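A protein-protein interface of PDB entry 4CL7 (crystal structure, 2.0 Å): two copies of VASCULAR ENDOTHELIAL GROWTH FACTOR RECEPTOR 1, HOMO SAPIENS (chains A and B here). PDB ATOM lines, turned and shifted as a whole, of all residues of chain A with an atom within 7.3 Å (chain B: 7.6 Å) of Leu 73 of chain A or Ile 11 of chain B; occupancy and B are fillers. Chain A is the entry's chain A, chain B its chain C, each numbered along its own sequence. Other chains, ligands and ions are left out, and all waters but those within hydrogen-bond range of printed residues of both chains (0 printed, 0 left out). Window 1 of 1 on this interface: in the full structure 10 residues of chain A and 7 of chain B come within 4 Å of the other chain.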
ATOM      1  N   SER A   9      -1.811 -23.134  21.451  1.00  0.00           N
ATOM      2  CA  SER A   9      -1.896 -24.391  20.720  1.00  0.00           C
ATOM      3  C   SER A   9      -3.305 -24.968  20.802  1.00  0.00           C
ATOM      4  O   SER A   9      -4.103 -24.815  19.876  1.00  0.00           O
ATOM      5  CB  SER A   9      -0.858 -25.390  21.231  1.00  0.00           C
ATOM      6  OG  SER A   9       0.459 -24.931  20.962  1.00  0.00           O
ATOM      7  N   PRO A  12      -6.991 -21.686  20.105  1.00  0.00           N
ATOM      8  CA  PRO A  12      -6.452 -20.540  19.361  1.00  0.00           C
ATOM      9  C   PRO A  12      -6.919 -19.209  19.935  1.00  0.00           C
ATOM     10  O   PRO A  12      -7.990 -19.120  20.525  1.00  0.00           O
ATOM     11  CB  PRO A  12      -7.015 -20.740  17.950  1.00  0.00           C
ATOM     12  CG  PRO A  12      -8.255 -21.548  18.151  1.00  0.00           C
ATOM     13  CD  PRO A  12      -7.977 -22.448  19.318  1.00  0.00           C
ATOM     14  N   GLU A  13      -6.100 -18.180  19.770  1.00  0.00           N
ATOM     15  CA  GLU A  13      -6.422 -16.853  20.250  1.00  0.00           C
ATOM     16  C   GLU A  13      -7.324 -16.153  19.225  1.00  0.00           C
ATOM     17  O   GLU A  13      -7.061 -16.194  18.028  1.00  0.00           O
ATOM     18  CB  GLU A  13      -5.125 -16.074  20.479  1.00  0.00           C
ATOM     19  CG  GLU A  13      -5.276 -14.570  20.561  1.00  0.00           C
ATOM     20  CD  GLU A  13      -5.666 -14.103  21.948  1.00  0.00           C
ATOM     21  OE1 GLU A  13      -6.112 -14.952  22.752  1.00  0.00           O
ATOM     22  OE2 GLU A  13      -5.518 -12.890  22.230  1.00  0.00           O
ATOM     23  N   LYS A  39       0.773 -19.649   8.020  1.00  0.00           N
ATOM     24  CA  LYS A  39      -0.018 -20.563   7.205  1.00  0.00           C
ATOM     25  C   LYS A  39      -1.480 -20.387   7.494  1.00  0.00           C
ATOM     26  O   LYS A  39      -1.845 -20.003   8.605  1.00  0.00           O
ATOM     27  CB  LYS A  39       0.381 -22.011   7.484  1.00  0.00           C
ATOM     28  CG  LYS A  39       1.694 -22.415   6.862  1.00  0.00           C
ATOM     29  CD  LYS A  39       2.061 -23.814   7.269  1.00  0.00           C
ATOM     30  CE  LYS A  39       3.274 -24.315   6.495  1.00  0.00           C
ATOM     31  NZ  LYS A  39       3.630 -25.716   6.880  1.00  0.00           N
ATOM     32  N   LYS A  40      -2.318 -20.656   6.494  1.00  0.00           N
ATOM     33  CA  LYS A  40      -3.755 -20.730   6.718  1.00  0.00           C
ATOM     34  C   LYS A  40      -4.221 -22.169   6.546  1.00  0.00           C
ATOM     35  O   LYS A  40      -3.963 -22.809   5.514  1.00  0.00           O
ATOM     36  CB  LYS A  40      -4.548 -19.794   5.800  1.00  0.00           C
ATOM     37  CG  LYS A  40      -6.044 -19.841   6.092  1.00  0.00           C
ATOM     38  CD  LYS A  40      -6.882 -19.220   4.992  1.00  0.00           C
ATOM     39  CE  LYS A  40      -8.366 -19.497   5.214  1.00  0.00           C
ATOM     40  NZ  LYS A  40      -9.186 -19.073   4.038  1.00  0.00           N
ATOM     41  N   PHE A  41      -4.889 -22.684   7.572  1.00  0.00           N
ATOM     42  CA  PHE A  41      -5.308 -24.081   7.581  1.00  0.00           C
ATOM     43  C   PHE A  41      -6.328 -24.337   6.482  1.00  0.00           C
ATOM     44  O   PHE A  41      -7.232 -23.542   6.289  1.00  0.00           O
ATOM     45  CB  PHE A  41      -5.910 -24.448   8.937  1.00  0.00           C
ATOM     46  CG  PHE A  41      -6.270 -25.903   9.066  1.00  0.00           C
ATOM     47  CD1 PHE A  41      -5.302 -26.842   9.390  1.00  0.00           C
ATOM     48  CD2 PHE A  41      -7.571 -26.331   8.860  1.00  0.00           C
ATOM     49  CE1 PHE A  41      -5.625 -28.188   9.506  1.00  0.00           C
ATOM     50  CE2 PHE A  41      -7.904 -27.675   8.976  1.00  0.00           C
ATOM     51  CZ  PHE A  41      -6.928 -28.605   9.300  1.00  0.00           C
ATOM     52  N   PRO A  42      -6.194 -25.466   5.771  1.00  0.00           N
ATOM     53  CA  PRO A  42      -5.129 -26.447   5.982  1.00  0.00           C
ATOM     54  C   PRO A  42      -4.078 -26.408   4.870  1.00  0.00           C
ATOM     55  O   PRO A  42      -3.136 -27.200   4.892  1.00  0.00           O
ATOM     56  CB  PRO A  42      -5.891 -27.769   5.903  1.00  0.00           C
ATOM     57  CG  PRO A  42      -6.931 -27.507   4.842  1.00  0.00           C
ATOM     58  CD  PRO A  42      -7.282 -26.017   4.941  1.00  0.00           C
ATOM     59  N   ASP A  44      -2.687 -23.257   2.823  1.00  0.00           N
ATOM     60  CA  ASP A  44      -1.950 -22.105   2.294  1.00  0.00           C
ATOM     61  C   ASP A  44      -0.761 -21.664   3.141  1.00  0.00           C
ATOM     62  O   ASP A  44      -0.793 -21.769   4.367  1.00  0.00           O
ATOM     63  CB  ASP A  44      -2.885 -20.896   2.140  1.00  0.00           C
ATOM     64  CG  ASP A  44      -4.159 -21.221   1.384  1.00  0.00           C
ATOM     65  OD1 ASP A  44      -4.073 -21.816   0.293  1.00  0.00           O
ATOM     66  OD2 ASP A  44      -5.253 -20.872   1.882  1.00  0.00           O
ATOM     67  N   GLU A  70      -8.342 -14.169   4.520  1.00  0.00           N
ATOM     68  CA  GLU A  70      -7.640 -14.218   5.808  1.00  0.00           C
ATOM     69  C   GLU A  70      -8.558 -14.547   6.983  1.00  0.00           C
ATOM     70  O   GLU A  70      -8.121 -14.510   8.138  1.00  0.00           O
ATOM     71  CB  GLU A  70      -6.942 -12.890   6.113  1.00  0.00           C
ATOM     72  CG  GLU A  70      -5.605 -12.710   5.425  1.00  0.00           C
ATOM     73  CD  GLU A  70      -5.748 -12.635   3.922  1.00  0.00           C
ATOM     74  OE1 GLU A  70      -6.451 -11.717   3.433  1.00  0.00           O
ATOM     75  OE2 GLU A  70      -5.174 -13.506   3.233  1.00  0.00           O
ATOM     76  N   ILE A  71      -9.831 -14.814   6.702  1.00  0.00           N
ATOM     77  CA  ILE A  71     -10.742 -15.288   7.741  1.00  0.00           C
ATOM     78  C   ILE A  71     -10.549 -16.786   7.964  1.00  0.00           C
ATOM     79  O   ILE A  71     -10.676 -17.573   7.040  1.00  0.00           O
ATOM     80  CB  ILE A  71     -12.219 -15.028   7.376  1.00  0.00           C
ATOM     81  CG1 ILE A  71     -12.506 -13.523   7.336  1.00  0.00           C
ATOM     82  CG2 ILE A  71     -13.127 -15.682   8.388  1.00  0.00           C
ATOM     83  CD1 ILE A  71     -13.833 -13.177   6.675  1.00  0.00           C
ATOM     84  N   GLY A  72     -10.240 -17.184   9.193  1.00  0.00           N
ATOM     85  CA  GLY A  72     -10.062 -18.593   9.480  1.00  0.00           C
ATOM     86  C   GLY A  72      -8.908 -18.833  10.431  1.00  0.00           C
ATOM     87  O   GLY A  72      -8.490 -17.930  11.155  1.00  0.00           O
ATOM     88  N   LEU A  73      -8.396 -20.058  10.420  1.00  0.00           N
ATOM     89  CA  LEU A  73      -7.346 -20.475  11.342  1.00  0.00           C
ATOM     90  C   LEU A  73      -5.992 -20.164  10.740  1.00  0.00           C
ATOM     91  O   LEU A  73      -5.579 -20.799   9.765  1.00  0.00           O
ATOM     92  CB  LEU A  73      -7.435 -21.983  11.594  1.00  0.00           C
ATOM     93  CG  LEU A  73      -6.342 -22.562  12.501  1.00  0.00           C
ATOM     94  CD1 LEU A  73      -6.495 -22.030  13.913  1.00  0.00           C
ATOM     95  CD2 LEU A  73      -6.354 -24.090  12.496  1.00  0.00           C
ATOM     96  N   LEU A  74      -5.303 -19.190  11.317  1.00  0.00           N
ATOM     97  CA  LEU A  74      -3.975 -18.835  10.859  1.00  0.00           C
ATOM     98  C   LEU A  74      -2.983 -19.428  11.849  1.00  0.00           C
ATOM     99  O   LEU A  74      -3.247 -19.447  13.047  1.00  0.00           O
ATOM    100  CB  LEU A  74      -3.842 -17.308  10.761  1.00  0.00           C
ATOM    101  CG  LEU A  74      -4.842 -16.647   9.812  1.00  0.00           C
ATOM    102  CD1 LEU A  74      -4.520 -15.179   9.621  1.00  0.00           C
ATOM    103  CD2 LEU A  74      -4.835 -17.344   8.479  1.00  0.00           C
ATOM    104  N   THR A  75      -1.866 -19.945  11.350  1.00  0.00           N
ATOM    105  CA  THR A  75      -0.857 -20.550  12.208  1.00  0.00           C
ATOM    106  C   THR A  75       0.535 -20.001  11.902  1.00  0.00           C
ATOM    107  O   THR A  75       0.933 -19.908  10.741  1.00  0.00           O
ATOM    108  CB  THR A  75      -0.840 -22.093  12.045  1.00  0.00           C
ATOM    109  OG1 THR A  75      -2.126 -22.629  12.385  1.00  0.00           O
ATOM    110  CG2 THR A  75       0.211 -22.710  12.946  1.00  0.00           C
ATOM    111  N   THR A  87       1.931 -21.696  16.860  1.00  0.00           N
ATOM    112  CA  THR A  87       0.964 -20.953  17.656  1.00  0.00           C
ATOM    113  C   THR A  87      -0.234 -20.576  16.763  1.00  0.00           C
ATOM    114  O   THR A  87      -0.059 -20.227  15.597  1.00  0.00           O
ATOM    115  CB  THR A  87       1.612 -19.735  18.370  1.00  0.00           C
ATOM    116  OG1 THR A  87       0.641 -19.080  19.190  1.00  0.00           O
ATOM    117  CG2 THR A  87       2.202 -18.737  17.369  1.00  0.00           C
ATOM    118  N   ASN A  88      -1.444 -20.681  17.304  1.00  0.00           N
ATOM    119  CA  ASN A  88      -2.663 -20.616  16.485  1.00  0.00           C
ATOM    120  C   ASN A  88      -3.570 -19.418  16.751  1.00  0.00           C
ATOM    121  O   ASN A  88      -3.864 -19.094  17.905  1.00  0.00           O
ATOM    122  CB  ASN A  88      -3.482 -21.899  16.671  1.00  0.00           C
ATOM    123  CG  ASN A  88      -2.717 -23.132  16.266  1.00  0.00           C
ATOM    124  OD1 ASN A  88      -2.343 -23.280  15.112  1.00  0.00           O
ATOM    125  ND2 ASN A  88      -2.477 -24.027  17.221  1.00  0.00           N
ATOM    126  N   TYR A  89      -4.044 -18.794  15.673  1.00  0.00           N
ATOM    127  CA  TYR A  89      -4.948 -17.645  15.763  1.00  0.00           C
ATOM    128  C   TYR A  89      -6.209 -17.879  14.926  1.00  0.00           C
ATOM    129  O   TYR A  89      -6.141 -18.381  13.809  1.00  0.00           O
ATOM    130  CB  TYR A  89      -4.234 -16.374  15.308  1.00  0.00           C
ATOM    131  CG  TYR A  89      -3.066 -16.032  16.202  1.00  0.00           C
ATOM    132  CD1 TYR A  89      -3.250 -15.285  17.357  1.00  0.00           C
ATOM    133  CD2 TYR A  89      -1.791 -16.507  15.925  1.00  0.00           C
ATOM    134  CE1 TYR A  89      -2.194 -14.999  18.197  1.00  0.00           C
ATOM    135  CE2 TYR A  89      -0.722 -16.217  16.764  1.00  0.00           C
ATOM    136  CZ  TYR A  89      -0.935 -15.466  17.898  1.00  0.00           C
ATOM    137  OH  TYR A  89       0.113 -15.163  18.742  1.00  0.00           O
ATOM    138  N   LEU A  90      -7.367 -17.526  15.471  1.00  0.00           N
ATOM    139  CA  LEU A  90      -8.611 -17.678  14.715  1.00  0.00           C
ATOM    140  C   LEU A  90      -9.187 -16.290  14.440  1.00  0.00           C
ATOM    141  O   LEU A  90      -9.629 -15.596  15.351  1.00  0.00           O
ATOM    142  CB  LEU A  90      -9.601 -18.538  15.493  1.00  0.00           C
ATOM    143  CG  LEU A  90     -10.864 -18.991  14.756  1.00  0.00           C
ATOM    144  CD1 LEU A  90     -10.509 -19.975  13.656  1.00  0.00           C
ATOM    145  CD2 LEU A  90     -11.836 -19.623  15.727  1.00  0.00           C
ATOM    146  N   THR A  91      -9.149 -15.868  13.188  1.00  0.00           N
ATOM    147  CA  THR A  91      -9.632 -14.538  12.867  1.00  0.00           C
ATOM    148  C   THR A  91     -11.136 -14.587  12.699  1.00  0.00           C
ATOM    149  O   THR A  91     -11.709 -15.624  12.359  1.00  0.00           O
ATOM    150  CB  THR A  91      -8.975 -13.986  11.606  1.00  0.00           C
ATOM    151  OG1 THR A  91      -9.227 -14.881  10.521  1.00  0.00           O
ATOM    152  CG2 THR A  91      -7.469 -13.856  11.813  1.00  0.00           C
ATOM    153  N   MET B   7     -21.115 -29.818  12.630  1.00  0.00           N
ATOM    154  CA  MET B   7     -20.010 -30.372  13.409  1.00  0.00           C
ATOM    155  C   MET B   7     -18.698 -29.620  13.230  1.00  0.00           C
ATOM    156  O   MET B   7     -18.121 -29.612  12.144  1.00  0.00           O
ATOM    157  CB  MET B   7     -19.809 -31.864  13.123  1.00  0.00           C
ATOM    158  CG  MET B   7     -19.115 -32.551  14.292  1.00  0.00           C
ATOM    159  SD  MET B   7     -18.876 -34.318  14.149  1.00  0.00           S
ATOM    160  CE  MET B   7     -20.560 -34.885  13.954  1.00  0.00           C
ATOM    161  N   TYR B   8     -18.230 -28.995  14.305  1.00  0.00           N
ATOM    162  CA  TYR B   8     -16.983 -28.243  14.239  1.00  0.00           C
ATOM    163  C   TYR B   8     -15.911 -28.962  15.034  1.00  0.00           C
ATOM    164  O   TYR B   8     -15.599 -28.573  16.155  1.00  0.00           O
ATOM    165  CB  TYR B   8     -17.183 -26.817  14.751  1.00  0.00           C
ATOM    166  CG  TYR B   8     -18.251 -26.097  13.984  1.00  0.00           C
ATOM    167  CD1 TYR B   8     -17.961 -25.491  12.771  1.00  0.00           C
ATOM    168  CD2 TYR B   8     -19.555 -26.044  14.450  1.00  0.00           C
ATOM    169  CE1 TYR B   8     -18.932 -24.838  12.050  1.00  0.00           C
ATOM    170  CE2 TYR B   8     -20.535 -25.389  13.735  1.00  0.00           C
ATOM    171  CZ  TYR B   8     -20.215 -24.791  12.531  1.00  0.00           C
ATOM    172  OH  TYR B   8     -21.180 -24.143  11.796  1.00  0.00           O
ATOM    173  N   SER B   9     -15.356 -30.004  14.426  1.00  0.00           N
ATOM    174  CA  SER B   9     -14.376 -30.879  15.063  1.00  0.00           C
ATOM    175  C   SER B   9     -12.963 -30.337  14.954  1.00  0.00           C
ATOM    176  O   SER B   9     -12.182 -30.431  15.898  1.00  0.00           O
ATOM    177  CB  SER B   9     -14.424 -32.267  14.419  1.00  0.00           C
ATOM    178  OG  SER B   9     -15.736 -32.793  14.451  1.00  0.00           O
ATOM    179  N   GLU B  10     -12.635 -29.778  13.794  1.00  0.00           N
ATOM    180  CA  GLU B  10     -11.282 -29.311  13.516  1.00  0.00           C
ATOM    181  C   GLU B  10     -11.038 -27.885  14.004  1.00  0.00           C
ATOM    182  O   GLU B  10     -10.098 -27.617  14.751  1.00  0.00           O
ATOM    183  CB  GLU B  10     -11.019 -29.374  12.012  1.00  0.00           C
ATOM    184  CG  GLU B  10     -11.004 -30.778  11.450  1.00  0.00           C
ATOM    185  CD  GLU B  10      -9.702 -31.498  11.738  1.00  0.00           C
ATOM    186  OE1 GLU B  10      -8.966 -31.048  12.643  1.00  0.00           O
ATOM    187  OE2 GLU B  10      -9.417 -32.507  11.056  1.00  0.00           O
ATOM    188  N   ILE B  11     -11.876 -26.970  13.539  1.00  0.00           N
ATOM    189  CA  ILE B  11     -11.789 -25.569  13.911  1.00  0.00           C
ATOM    190  C   ILE B  11     -13.094 -25.185  14.603  1.00  0.00           C
ATOM    191  O   ILE B  11     -14.174 -25.419  14.054  1.00  0.00           O
ATOM    192  CB  ILE B  11     -11.614 -24.701  12.663  1.00  0.00           C
ATOM    193  CG1 ILE B  11     -10.438 -25.214  11.822  1.00  0.00           C
ATOM    194  CG2 ILE B  11     -11.445 -23.235  13.051  1.00  0.00           C
ATOM    195  CD1 ILE B  11     -10.238 -24.461  10.526  1.00  0.00           C
ATOM    196  N   PRO B  12     -13.008 -24.626  15.818  1.00  0.00           N
ATOM    197  CA  PRO B  12     -14.236 -24.317  16.554  1.00  0.00           C
ATOM    198  C   PRO B  12     -15.031 -23.229  15.874  1.00  0.00           C
ATOM    199  O   PRO B  12     -14.463 -22.364  15.204  1.00  0.00           O
ATOM    200  CB  PRO B  12     -13.726 -23.799  17.901  1.00  0.00           C
ATOM    201  CG  PRO B  12     -12.343 -24.340  18.014  1.00  0.00           C
ATOM    202  CD  PRO B  12     -11.809 -24.332  16.617  1.00  0.00           C
ATOM    203  N   GLU B  13     -16.341 -23.281  16.053  1.00  0.00           N
ATOM    204  CA  GLU B  13     -17.215 -22.205  15.629  1.00  0.00           C
ATOM    205  C   GLU B  13     -17.180 -21.087  16.679  1.00  0.00           C
ATOM    206  O   GLU B  13     -17.233 -21.351  17.873  1.00  0.00           O
ATOM    207  CB  GLU B  13     -18.635 -22.744  15.457  1.00  0.00           C
ATOM    208  CG  GLU B  13     -19.705 -21.687  15.241  1.00  0.00           C
ATOM    209  CD  GLU B  13     -19.790 -21.229  13.803  1.00  0.00           C
ATOM    210  OE1 GLU B  13     -18.757 -21.267  13.098  1.00  0.00           O
ATOM    211  OE2 GLU B  13     -20.900 -20.843  13.374  1.00  0.00           O
ATOM    212  N   ILE B  14     -17.080 -19.837  16.240  1.00  0.00           N
ATOM    213  CA  ILE B  14     -17.134 -18.723  17.180  1.00  0.00           C
ATOM    214  C   ILE B  14     -18.573 -18.310  17.461  1.00  0.00           C
ATOM    215  O   ILE B  14     -19.368 -18.116  16.534  1.00  0.00           O
ATOM    216  CB  ILE B  14     -16.338 -17.500  16.668  1.00  0.00           C
ATOM    217  CG1 ILE B  14     -14.841 -17.833  16.631  1.00  0.00           C
ATOM    218  CG2 ILE B  14     -16.609 -16.280  17.550  1.00  0.00           C
ATOM    219  CD1 ILE B  14     -13.972 -16.750  16.013  1.00  0.00           C
ATOM    220  N   THR B  87     -17.887 -31.517  18.854  1.00  0.00           N
ATOM    221  CA  THR B  87     -18.098 -30.268  18.152  1.00  0.00           C
ATOM    222  C   THR B  87     -17.761 -29.125  19.112  1.00  0.00           C
ATOM    223  O   THR B  87     -18.173 -29.137  20.276  1.00  0.00           O
ATOM    224  CB  THR B  87     -19.522 -30.156  17.551  1.00  0.00           C
ATOM    225  OG1 THR B  87     -19.607 -28.988  16.721  1.00  0.00           O
ATOM    226  CG2 THR B  87     -20.566 -30.096  18.646  1.00  0.00           C
ATOM    227  N   ASN B  88     -16.987 -28.163  18.616  1.00  0.00           N
ATOM    228  CA  ASN B  88     -16.332 -27.164  19.459  1.00  0.00           C
ATOM    229  C   ASN B  88     -16.768 -25.728  19.185  1.00  0.00           C
ATOM    230  O   ASN B  88     -16.890 -25.311  18.030  1.00  0.00           O
ATOM    231  CB  ASN B  88     -14.808 -27.263  19.298  1.00  0.00           C
ATOM    232  CG  ASN B  88     -14.272 -28.635  19.670  1.00  0.00           C
ATOM    233  OD1 ASN B  88     -14.065 -28.929  20.846  1.00  0.00           O
ATOM    234  ND2 ASN B  88     -14.064 -29.489  18.664  1.00  0.00           N
ATOM    235  N   TYR B  89     -16.985 -24.976  20.260  1.00  0.00           N
ATOM    236  CA  TYR B  89     -17.400 -23.583  20.177  1.00  0.00           C
ATOM    237  C   TYR B  89     -16.505 -22.729  21.062  1.00  0.00           C
ATOM    238  O   TYR B  89     -16.187 -23.107  22.190  1.00  0.00           O
ATOM    239  CB  TYR B  89     -18.863 -23.420  20.595  1.00  0.00           C
ATOM    240  CG  TYR B  89     -19.791 -24.285  19.777  1.00  0.00           C
ATOM    241  CD1 TYR B  89     -20.060 -25.594  20.156  1.00  0.00           C
ATOM    242  CD2 TYR B  89     -20.367 -23.811  18.605  1.00  0.00           C
ATOM    243  CE1 TYR B  89     -20.880 -26.398  19.405  1.00  0.00           C
ATOM    244  CE2 TYR B  89     -21.194 -24.622  17.841  1.00  0.00           C
ATOM    245  CZ  TYR B  89     -21.446 -25.914  18.254  1.00  0.00           C
ATOM    246  OH  TYR B  89     -22.265 -26.737  17.513  1.00  0.00           O
ATOM    247  N   LEU B  90     -16.096 -21.583  20.531  1.00  0.00           N
ATOM    248  CA  LEU B  90     -15.311 -20.614  21.278  1.00  0.00           C
ATOM    249  C   LEU B  90     -16.164 -19.382  21.530  1.00  0.00           C
ATOM    250  O   LEU B  90     -16.540 -18.685  20.595  1.00  0.00           O
ATOM    251  CB  LEU B  90     -14.090 -20.210  20.457  1.00  0.00           C
ATOM    252  CG  LEU B  90     -12.934 -21.209  20.455  1.00  0.00           C
ATOM    253  CD1 LEU B  90     -11.928 -20.877  19.356  1.00  0.00           C
ATOM    254  CD2 LEU B  90     -12.265 -21.208  21.822  1.00  0.00           C
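Pro 12 of chain A touches Leu 90 of chain B, and with the chains exchanged Leu 90 of chain A touches Pro 12 of chain B. Leu 90 of chain B touches its own counterpart, Leu 90 of chain A. Of the 7 pairs that touch across the chains among the printed residues, 3 have their exchanged pair printed and touching as well.
Printed residues of chain B that touch a printed residue of chain A: Ile 11, Pro 12, Ile 14 and Leu 90. Of the 19 printed residues of chain A, 4 touch a printed residue of chain B. Hydrophobic or aromatic side chains of chain A within 4 Å of the printed part of chain B: Pro 12, Phe 41, Leu 73 and Leu 90. Among the printed residues, no Asp or Glu carboxylate lies within 4 Å of a Lys or Arg side-chain nitrogen of the other chain.
Lys 40 of chain A touches none of the printed residues of chain B. Of the printed residues of chain B, Phe 41 of chain A touches Ile 11. Of chain B, only Ile 11 (3.9 Å) comes within 4 Å of Leu 73 of chain A. Printed residues of chain B within 4 Å of Leu 90 of chain A: Ile 11 (3.4 Å), Pro 12 (3.8 Å), Ile 14 (3.6 Å) and Leu 90 (3.8 Å). Ile 11 of chain B touches three residues of chain A. Printed residues of chain A within 4 Å of Pro 12 of chain B: Leu 90. Printed residues of chain A within 4 Å of Ile 14 of chain B: Leu 90 (3.6 Å). Of the printed residues of chain A, Leu 90 of chain B touches Pro 12 (3.9 Å) and Leu 90 (3.8 Å). The nearest residue of chain B that does not touch Leu 73 of chain A is Glu 10 of chain B (5.6 Å). The nearest residue of chain A that does not touch Ile 11 of chain B is Gly 72 of chain A (5.7 Å). The nearest printed residue of chain A that does not touch Ile 14 of chain B is Thr 91 of chain A (4.4 Å).
O of Glu 13 of chain A lies within hydrogen-bond range of N of Leu 90 of chain A (2.9 Å). N of Phe 41 of chain A is in hydrogen-bond range of O of Leu 73 of chain A (3.0 Å). The backbone carbonyl oxygen of Glu 13 of chain B is in hydrogen-bond range of the backbone NH of Leu 90 of chain B (2.9 Å).
Pro 12 of chain A touches Leu 90 of chain B. CD2 of Phe 41 of chain A touches CD1 of Ile 11 of chain B (3.7 Å). Leu 73 of chain A touches Ile 11 of chain B (CB to CD1, 3.9 Å). Leu 90 of chain A touches Ile 11 of chain B (CD1 to CG2, 3.4 Å). CD2 of Leu 90 of chain A touches O of Pro 12 of chain B (3.8 Å). CD2 of Leu 90 of chain A touches CD1 of Ile 14 of chain B, 3.6 Å away. CD2 of Leu 90 of chain A touches CD1 of Leu 90 of chain B (3.8 Å).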
